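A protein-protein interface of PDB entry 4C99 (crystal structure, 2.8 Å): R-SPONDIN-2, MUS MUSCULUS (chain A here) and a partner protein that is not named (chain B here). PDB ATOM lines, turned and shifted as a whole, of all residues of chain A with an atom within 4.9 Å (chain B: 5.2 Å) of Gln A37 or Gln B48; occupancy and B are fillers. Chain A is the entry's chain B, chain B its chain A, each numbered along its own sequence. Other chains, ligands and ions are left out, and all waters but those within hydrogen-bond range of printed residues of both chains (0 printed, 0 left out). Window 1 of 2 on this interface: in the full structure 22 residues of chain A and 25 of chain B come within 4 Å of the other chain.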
ATOM      1  N   ASP A  16     -13.433  18.977  -0.433  1.00  0.00           N
ATOM      2  CA  ASP A  16     -14.760  19.427  -0.795  1.00  0.00           C
ATOM      3  C   ASP A  16     -14.804  20.734  -1.476  1.00  0.00           C
ATOM      4  O   ASP A  16     -15.754  21.010  -2.204  1.00  0.00           O
ATOM      5  CB  ASP A  16     -15.611  19.553   0.451  1.00  0.00           C
ATOM      6  CG  ASP A  16     -15.989  18.221   0.992  1.00  0.00           C
ATOM      7  OD1 ASP A  16     -16.559  17.453   0.174  1.00  0.00           O
ATOM      8  OD2 ASP A  16     -15.686  17.962   2.194  1.00  0.00           O
ATOM      9  N   ASN A  17     -13.800  21.553  -1.209  1.00  0.00           N
ATOM     10  CA  ASN A  17     -13.801  22.922  -1.678  1.00  0.00           C
ATOM     11  C   ASN A  17     -12.539  23.251  -2.443  1.00  0.00           C
ATOM     12  O   ASN A  17     -12.169  24.409  -2.567  1.00  0.00           O
ATOM     13  CB  ASN A  17     -13.952  23.831  -0.473  1.00  0.00           C
ATOM     14  CG  ASN A  17     -15.350  23.834   0.050  1.00  0.00           C
ATOM     15  OD1 ASN A  17     -16.312  23.717  -0.705  1.00  0.00           O
ATOM     16  ND2 ASN A  17     -15.486  24.023   1.340  1.00  0.00           N
ATOM     17  N   LEU A  30     -12.993  29.929  -9.245  1.00  0.00           N
ATOM     18  CA  LEU A  30     -14.082  29.028  -8.910  1.00  0.00           C
ATOM     19  C   LEU A  30     -14.384  28.304 -10.190  1.00  0.00           C
ATOM     20  O   LEU A  30     -14.605  28.953 -11.197  1.00  0.00           O
ATOM     21  CB  LEU A  30     -15.264  29.791  -8.361  1.00  0.00           C
ATOM     22  CG  LEU A  30     -14.888  30.348  -6.990  1.00  0.00           C
ATOM     23  CD1 LEU A  30     -16.000  31.125  -6.304  1.00  0.00           C
ATOM     24  CD2 LEU A  30     -14.461  29.207  -6.075  1.00  0.00           C
ATOM     25  N   ARG A  31     -14.238  26.980 -10.195  1.00  0.00           N
ATOM     26  CA  ARG A  31     -14.644  26.165 -11.342  1.00  0.00           C
ATOM     27  C   ARG A  31     -15.914  25.409 -10.961  1.00  0.00           C
ATOM     28  O   ARG A  31     -16.178  25.181  -9.790  1.00  0.00           O
ATOM     29  CB  ARG A  31     -13.553  25.190 -11.775  1.00  0.00           C
ATOM     30  CG  ARG A  31     -13.790  24.630 -13.181  1.00  0.00           C
ATOM     31  CD  ARG A  31     -12.738  23.623 -13.614  1.00  0.00           C
ATOM     32  NE  ARG A  31     -11.388  24.164 -13.484  1.00  0.00           N
ATOM     33  CZ  ARG A  31     -10.273  23.441 -13.544  1.00  0.00           C
ATOM     34  NH1 ARG A  31     -10.317  22.125 -13.749  1.00  0.00           N
ATOM     35  NH2 ARG A  31      -9.100  24.040 -13.403  1.00  0.00           N
ATOM     36  N   ARG A  32     -16.704  25.037 -11.958  1.00  0.00           N
ATOM     37  CA  ARG A  32     -18.025  24.479 -11.738  1.00  0.00           C
ATOM     38  C   ARG A  32     -18.132  23.182 -12.527  1.00  0.00           C
ATOM     39  O   ARG A  32     -17.843  23.140 -13.733  1.00  0.00           O
ATOM     40  CB  ARG A  32     -19.052  25.495 -12.193  1.00  0.00           C
ATOM     41  CG  ARG A  32     -20.478  25.008 -12.323  1.00  0.00           C
ATOM     42  CD  ARG A  32     -21.143  24.825 -10.980  1.00  0.00           C
ATOM     43  NE  ARG A  32     -21.509  26.056 -10.266  1.00  0.00           N
ATOM     44  CZ  ARG A  32     -21.820  26.090  -8.964  1.00  0.00           C
ATOM     45  NH1 ARG A  32     -21.793  24.983  -8.228  1.00  0.00           N
ATOM     46  NH2 ARG A  32     -22.118  27.231  -8.365  1.00  0.00           N
ATOM     47  N   MET A  35     -23.096  20.318  -9.901  1.00  0.00           N
ATOM     48  CA  MET A  35     -23.473  21.056  -8.705  1.00  0.00           C
ATOM     49  C   MET A  35     -22.252  21.388  -7.853  1.00  0.00           C
ATOM     50  O   MET A  35     -22.359  21.979  -6.776  1.00  0.00           O
ATOM     51  CB  MET A  35     -24.488  20.251  -7.916  1.00  0.00           C
ATOM     52  CG  MET A  35     -24.085  18.822  -7.665  1.00  0.00           C
ATOM     53  SD  MET A  35     -25.174  18.080  -6.429  1.00  0.00           S
ATOM     54  CE  MET A  35     -24.778  16.345  -6.687  1.00  0.00           C
ATOM     55  N   ARG A  36     -21.084  21.026  -8.364  1.00  0.00           N
ATOM     56  CA  ARG A  36     -19.845  21.078  -7.613  1.00  0.00           C
ATOM     57  C   ARG A  36     -19.155  22.400  -7.896  1.00  0.00           C
ATOM     58  O   ARG A  36     -19.231  22.923  -8.989  1.00  0.00           O
ATOM     59  CB  ARG A  36     -18.982  19.925  -8.074  1.00  0.00           C
ATOM     60  CG  ARG A  36     -18.057  19.307  -7.040  1.00  0.00           C
ATOM     61  CD  ARG A  36     -17.334  18.138  -7.704  1.00  0.00           C
ATOM     62  NE  ARG A  36     -18.313  17.317  -8.432  1.00  0.00           N
ATOM     63  CZ  ARG A  36     -18.058  16.582  -9.511  1.00  0.00           C
ATOM     64  NH1 ARG A  36     -16.844  16.530 -10.038  1.00  0.00           N
ATOM     65  NH2 ARG A  36     -19.047  15.895 -10.072  1.00  0.00           N
ATOM     66  N   GLN A  37     -18.518  22.966  -6.891  1.00  0.00           N
ATOM     67  CA  GLN A  37     -17.703  24.161  -7.074  1.00  0.00           C
ATOM     68  C   GLN A  37     -16.577  24.151  -6.081  1.00  0.00           C
ATOM     69  O   GLN A  37     -16.812  24.128  -4.835  1.00  0.00           O
ATOM     70  CB  GLN A  37     -18.502  25.410  -6.859  1.00  0.00           C
ATOM     71  CG  GLN A  37     -17.668  26.650  -7.010  1.00  0.00           C
ATOM     72  CD  GLN A  37     -18.296  27.837  -6.335  1.00  0.00           C
ATOM     73  OE1 GLN A  37     -18.565  27.787  -5.146  1.00  0.00           O
ATOM     74  NE2 GLN A  37     -18.526  28.915  -7.084  1.00  0.00           N
ATOM     75  N   TYR A  38     -15.368  24.157  -6.646  1.00  0.00           N
ATOM     76  CA  TYR A  38     -14.138  24.075  -5.878  1.00  0.00           C
ATOM     77  C   TYR A  38     -13.127  25.087  -6.426  1.00  0.00           C
ATOM     78  O   TYR A  38     -13.133  25.382  -7.618  1.00  0.00           O
ATOM     79  CB  TYR A  38     -13.594  22.656  -5.954  1.00  0.00           C
ATOM     80  CG  TYR A  38     -13.279  22.197  -7.384  1.00  0.00           C
ATOM     81  CD1 TYR A  38     -12.086  22.545  -8.002  1.00  0.00           C
ATOM     82  CD2 TYR A  38     -14.170  21.409  -8.100  1.00  0.00           C
ATOM     83  CE1 TYR A  38     -11.800  22.125  -9.293  1.00  0.00           C
ATOM     84  CE2 TYR A  38     -13.893  20.993  -9.391  1.00  0.00           C
ATOM     85  CZ  TYR A  38     -12.712  21.363  -9.981  1.00  0.00           C
ATOM     86  OH  TYR A  38     -12.435  20.983 -11.267  1.00  0.00           O
ATOM     87  N   GLY A  39     -12.255  25.602  -5.561  1.00  0.00           N
ATOM     88  CA  GLY A  39     -11.166  26.510  -5.987  1.00  0.00           C
ATOM     89  C   GLY A  39     -10.056  25.891  -6.859  1.00  0.00           C
ATOM     90  O   GLY A  39      -9.594  24.808  -6.596  1.00  0.00           O
ATOM     91  N   ILE B  46     -29.718  20.933  -5.849  1.00  0.00           N
ATOM     92  CA  ILE B  46     -28.658  21.306  -4.960  1.00  0.00           C
ATOM     93  C   ILE B  46     -27.621  22.039  -5.715  1.00  0.00           C
ATOM     94  O   ILE B  46     -27.378  21.704  -6.839  1.00  0.00           O
ATOM     95  CB  ILE B  46     -28.000  20.067  -4.355  1.00  0.00           C
ATOM     96  CG1 ILE B  46     -28.868  19.560  -3.203  1.00  0.00           C
ATOM     97  CG2 ILE B  46     -26.597  20.372  -3.877  1.00  0.00           C
ATOM     98  CD1 ILE B  46     -28.265  18.400  -2.435  1.00  0.00           C
ATOM     99  N   VAL B  47     -26.996  23.028  -5.085  1.00  0.00           N
ATOM    100  CA  VAL B  47     -25.900  23.744  -5.681  1.00  0.00           C
ATOM    101  C   VAL B  47     -24.873  23.947  -4.617  1.00  0.00           C
ATOM    102  O   VAL B  47     -25.218  24.503  -3.600  1.00  0.00           O
ATOM    103  CB  VAL B  47     -26.364  25.122  -6.197  1.00  0.00           C
ATOM    104  CG1 VAL B  47     -25.193  25.973  -6.645  1.00  0.00           C
ATOM    105  CG2 VAL B  47     -27.310  24.954  -7.356  1.00  0.00           C
ATOM    106  N   GLN B  48     -23.636  23.486  -4.848  1.00  0.00           N
ATOM    107  CA  GLN B  48     -22.537  23.629  -3.885  1.00  0.00           C
ATOM    108  C   GLN B  48     -22.049  24.988  -4.151  1.00  0.00           C
ATOM    109  O   GLN B  48     -22.001  25.387  -5.314  1.00  0.00           O
ATOM    110  CB  GLN B  48     -21.363  22.666  -4.157  1.00  0.00           C
ATOM    111  CG  GLN B  48     -20.366  22.604  -3.006  1.00  0.00           C
ATOM    112  CD  GLN B  48     -19.055  21.819  -3.244  1.00  0.00           C
ATOM    113  OE1 GLN B  48     -18.946  20.932  -4.078  1.00  0.00           O
ATOM    114  NE2 GLN B  48     -18.047  22.169  -2.478  1.00  0.00           N
ATOM    115  N   MET B  49     -21.691  25.702  -3.088  1.00  0.00           N
ATOM    116  CA  MET B  49     -21.026  27.002  -3.201  1.00  0.00           C
ATOM    117  C   MET B  49     -19.812  27.032  -2.298  1.00  0.00           C
ATOM    118  O   MET B  49     -19.922  26.773  -1.089  1.00  0.00           O
ATOM    119  CB  MET B  49     -21.946  28.091  -2.737  1.00  0.00           C
ATOM    120  CG  MET B  49     -23.247  28.137  -3.482  1.00  0.00           C
ATOM    121  SD  MET B  49     -22.926  28.781  -5.118  1.00  0.00           S
ATOM    122  CE  MET B  49     -22.898  30.527  -4.756  1.00  0.00           C
ATOM    123  N   HIS B  50     -18.655  27.352  -2.879  1.00  0.00           N
ATOM    124  CA  HIS B  50     -17.416  27.613  -2.128  1.00  0.00           C
ATOM    125  C   HIS B  50     -17.705  28.829  -1.277  1.00  0.00           C
ATOM    126  O   HIS B  50     -18.454  29.683  -1.703  1.00  0.00           O
ATOM    127  CB  HIS B  50     -16.289  27.928  -3.095  1.00  0.00           C
ATOM    128  CG  HIS B  50     -14.917  27.671  -2.558  1.00  0.00           C
ATOM    129  ND1 HIS B  50     -14.398  28.349  -1.479  1.00  0.00           N
ATOM    130  CD2 HIS B  50     -13.926  26.868  -3.017  1.00  0.00           C
ATOM    131  CE1 HIS B  50     -13.160  27.942  -1.266  1.00  0.00           C
ATOM    132  NE2 HIS B  50     -12.848  27.046  -2.188  1.00  0.00           N
ATOM    133  N   GLY B  53     -17.103  32.116  -2.491  1.00  0.00           N
ATOM    134  CA  GLY B  53     -17.943  32.370  -3.641  1.00  0.00           C
ATOM    135  C   GLY B  53     -19.182  33.099  -3.182  1.00  0.00           C
ATOM    136  O   GLY B  53     -20.151  33.270  -3.928  1.00  0.00           O
ATOM    137  N   TYR B  64     -27.750  31.663 -11.400  1.00  0.00           N
ATOM    138  CA  TYR B  64     -28.368  30.369 -11.093  1.00  0.00           C
ATOM    139  C   TYR B  64     -29.892  30.379 -11.182  1.00  0.00           C
ATOM    140  O   TYR B  64     -30.558  31.280 -10.677  1.00  0.00           O
ATOM    141  CB  TYR B  64     -27.953  29.899  -9.699  1.00  0.00           C
ATOM    142  CG  TYR B  64     -26.460  29.788  -9.549  1.00  0.00           C
ATOM    143  CD1 TYR B  64     -25.718  28.905 -10.344  1.00  0.00           C
ATOM    144  CD2 TYR B  64     -25.782  30.579  -8.656  1.00  0.00           C
ATOM    145  CE1 TYR B  64     -24.335  28.821 -10.239  1.00  0.00           C
ATOM    146  CE2 TYR B  64     -24.413  30.491  -8.532  1.00  0.00           C
ATOM    147  CZ  TYR B  64     -23.688  29.619  -9.323  1.00  0.00           C
ATOM    148  OH  TYR B  64     -22.313  29.547  -9.183  1.00  0.00           O
ATOM    149  N   VAL B  71     -25.555  24.545  -0.566  1.00  0.00           N
ATOM    150  CA  VAL B  71     -24.883  23.615   0.299  1.00  0.00           C
ATOM    151  C   VAL B  71     -23.437  24.092   0.395  1.00  0.00           C
ATOM    152  O   VAL B  71     -22.704  24.131  -0.612  1.00  0.00           O
ATOM    153  CB  VAL B  71     -24.933  22.205  -0.279  1.00  0.00           C
ATOM    154  CG1 VAL B  71     -24.381  21.213   0.719  1.00  0.00           C
ATOM    155  CG2 VAL B  71     -26.358  21.807  -0.625  1.00  0.00           C
ATOM    156  N   LYS B  73     -19.972  23.859   2.483  1.00  0.00           N
ATOM    157  CA  LYS B  73     -18.892  23.308   3.325  1.00  0.00           C
ATOM    158  C   LYS B  73     -17.848  24.370   3.787  1.00  0.00           C
ATOM    159  O   LYS B  73     -16.913  24.734   3.041  1.00  0.00           O
ATOM    160  CB  LYS B  73     -18.191  22.147   2.558  1.00  0.00           C
ATOM    161  CG  LYS B  73     -16.933  21.541   3.185  1.00  0.00           C
ATOM    162  CD  LYS B  73     -17.255  20.768   4.435  1.00  0.00           C
ATOM    163  CE  LYS B  73     -16.022  20.526   5.275  1.00  0.00           C
ATOM    164  NZ  LYS B  73     -16.463  20.083   6.630  1.00  0.00           N
ATOM    165  N   VAL B 143     -22.786  14.972  -2.839  1.00  0.00           N
ATOM    166  CA  VAL B 143     -22.481  16.203  -3.548  1.00  0.00           C
ATOM    167  C   VAL B 143     -21.154  16.125  -4.290  1.00  0.00           C
ATOM    168  O   VAL B 143     -21.049  16.491  -5.452  1.00  0.00           O
ATOM    169  CB  VAL B 143     -22.368  17.393  -2.591  1.00  0.00           C
ATOM    170  CG1 VAL B 143     -21.953  18.609  -3.384  1.00  0.00           C
ATOM    171  CG2 VAL B 143     -23.683  17.664  -1.896  1.00  0.00           C
ATOM    172  N   ASN B 144     -20.141  15.665  -3.590  1.00  0.00           N
ATOM    173  CA  ASN B 144     -18.823  15.489  -4.156  1.00  0.00           C
ATOM    174  C   ASN B 144     -18.781  14.612  -5.393  1.00  0.00           C
ATOM    175  O   ASN B 144     -18.032  14.897  -6.307  1.00  0.00           O
ATOM    176  CB  ASN B 144     -17.909  14.840  -3.119  1.00  0.00           C
ATOM    177  CG  ASN B 144     -16.689  15.658  -2.839  1.00  0.00           C
ATOM    178  OD1 ASN B 144     -15.570  15.255  -3.176  1.00  0.00           O
ATOM    179  ND2 ASN B 144     -16.892  16.828  -2.222  1.00  0.00           N
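The backbone NH (N) of Gln B48 lies within hydrogen-bond range of the backbone carbonyl oxygen (O) of Met A35 (2.8 Å). NE2 of Gln B48 is in hydrogen-bond range of O of Asp A16. NE2 of Gln B48 lies within hydrogen-bond range of OD1 of Asn A17, 2.9 Å away. The side-chain hydroxyl (OH) of Tyr B64 is in hydrogen-bond range of the guanidinium group (NH2) of Arg A32, at 2.5 Å. The backbone carbonyl oxygen (O) of Gln B48 sits at hydrogen-bond distance from the guanidinium group (NH1) of Arg A32. The side-chain sulfur (SD) of Met B49 is in hydrogen-bond range of the guanidinium group (NH2) of Arg A32 (3.7 Å). OD1 of Asp A16 is in hydrogen-bond range of ND2 of Asn B144, at 2.5 Å. The backbone carbonyl oxygen of Gln A37 is in hydrogen-bond range of the side-chain amide nitrogen of Gln B48 (3.3 Å). ND2 of Asn A17 lies close to O of Lys B73 (2.3 Å). The backbone carbonyl oxygen of Asn B144 is in hydrogen-bond range of the guanidinium group of Arg A36 (3.2 Å). The backbone NH of His B50 sits close to the side-chain amide oxygen of Gln A37 (2.3 Å). The backbone carbonyl oxygen (O) of Asn A17 is in hydrogen-bond range of a ring nitrogen (NE2) of His B50, at 2.7 Å.
The backbone NH (N) of Gly A39 lies within hydrogen-bond range of the backbone carbonyl oxygen (O) of Asn A17, 3.2 Å away. The backbone carbonyl oxygen (O) of Tyr A38 sits at hydrogen-bond distance from the backbone NH (N) of Arg A31 (3.2 Å). O of Arg A36 sits close to NH1 of Arg A32 (3.4 Å). O of Val B71 sits at hydrogen-bond distance from N of Met B49 (3.1 Å). The guanidinium group of Arg A32 sits at hydrogen-bond distance from the backbone carbonyl oxygen of Met A35, at 3.4 Å. N of Val B71 is in hydrogen-bond range of O of Val B47 (3.1 Å).
CG of Lys B73 touches CB of Asp A16, 3.6 Å away. CD2 of Leu A30 touches CB of His B50, at 3.7 Å. CD1 of Leu A30 touches CA of Gly B53, 3.5 Å away. Arg A32 touches Val B47. O of Ile B46 touches CB of Met A35 (3.4 Å). Met A35 touches Val B47 (O to C, 3.9 Å). CA of Val B143 touches CE of Met A35 (3.9 Å). Gln B48 touches Arg A36 (OE1 to CG, 3.5 Å). OE1 of Gln A37 touches C of Met B49 (3.2 Å). Gly A39 touches His B50 (N to CD2, 3.3 Å).
Of chain B, only Gln B48 (3.3 Å), Met B49 (3.2 Å) and His B50 (2.3 Å) come within 4 Å of Gln A37. Gln B48 touches just these residues of chain A: Asp A16, Asn A17, Arg A32, Met A35, Arg A36 and Gln A37. Printed residues of chain A within 4 Å of Met B49: Arg A32 and Gln A37. Printed residues of chain A within 4 Å of Gly B53: Leu A30. Arg A31 touches none of the printed residues of chain B. Val B71 touches none of the printed residues of chain A.
Of the 10 printed residues of chain A, 9 touch a printed residue of chain B. Printed residues of chain B that touch a printed residue of chain A: Ile B46, Val B47, Gln B48, Met B49, His B50, Gly B53, Tyr B64, Lys B73, Val B143 and Asn B144. Hydrophobic or aromatic side chains of chain B within 4 Å of the printed part of chain A: Ile B46, Val B47, Met B49, His B50 and Tyr B64. Among the printed residues, 23 pairs touch across the chains. Among the printed residues, no Asp or Glu carboxylate lies within 4 Å of a Lys or Arg side-chain nitrogen of the other chain.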
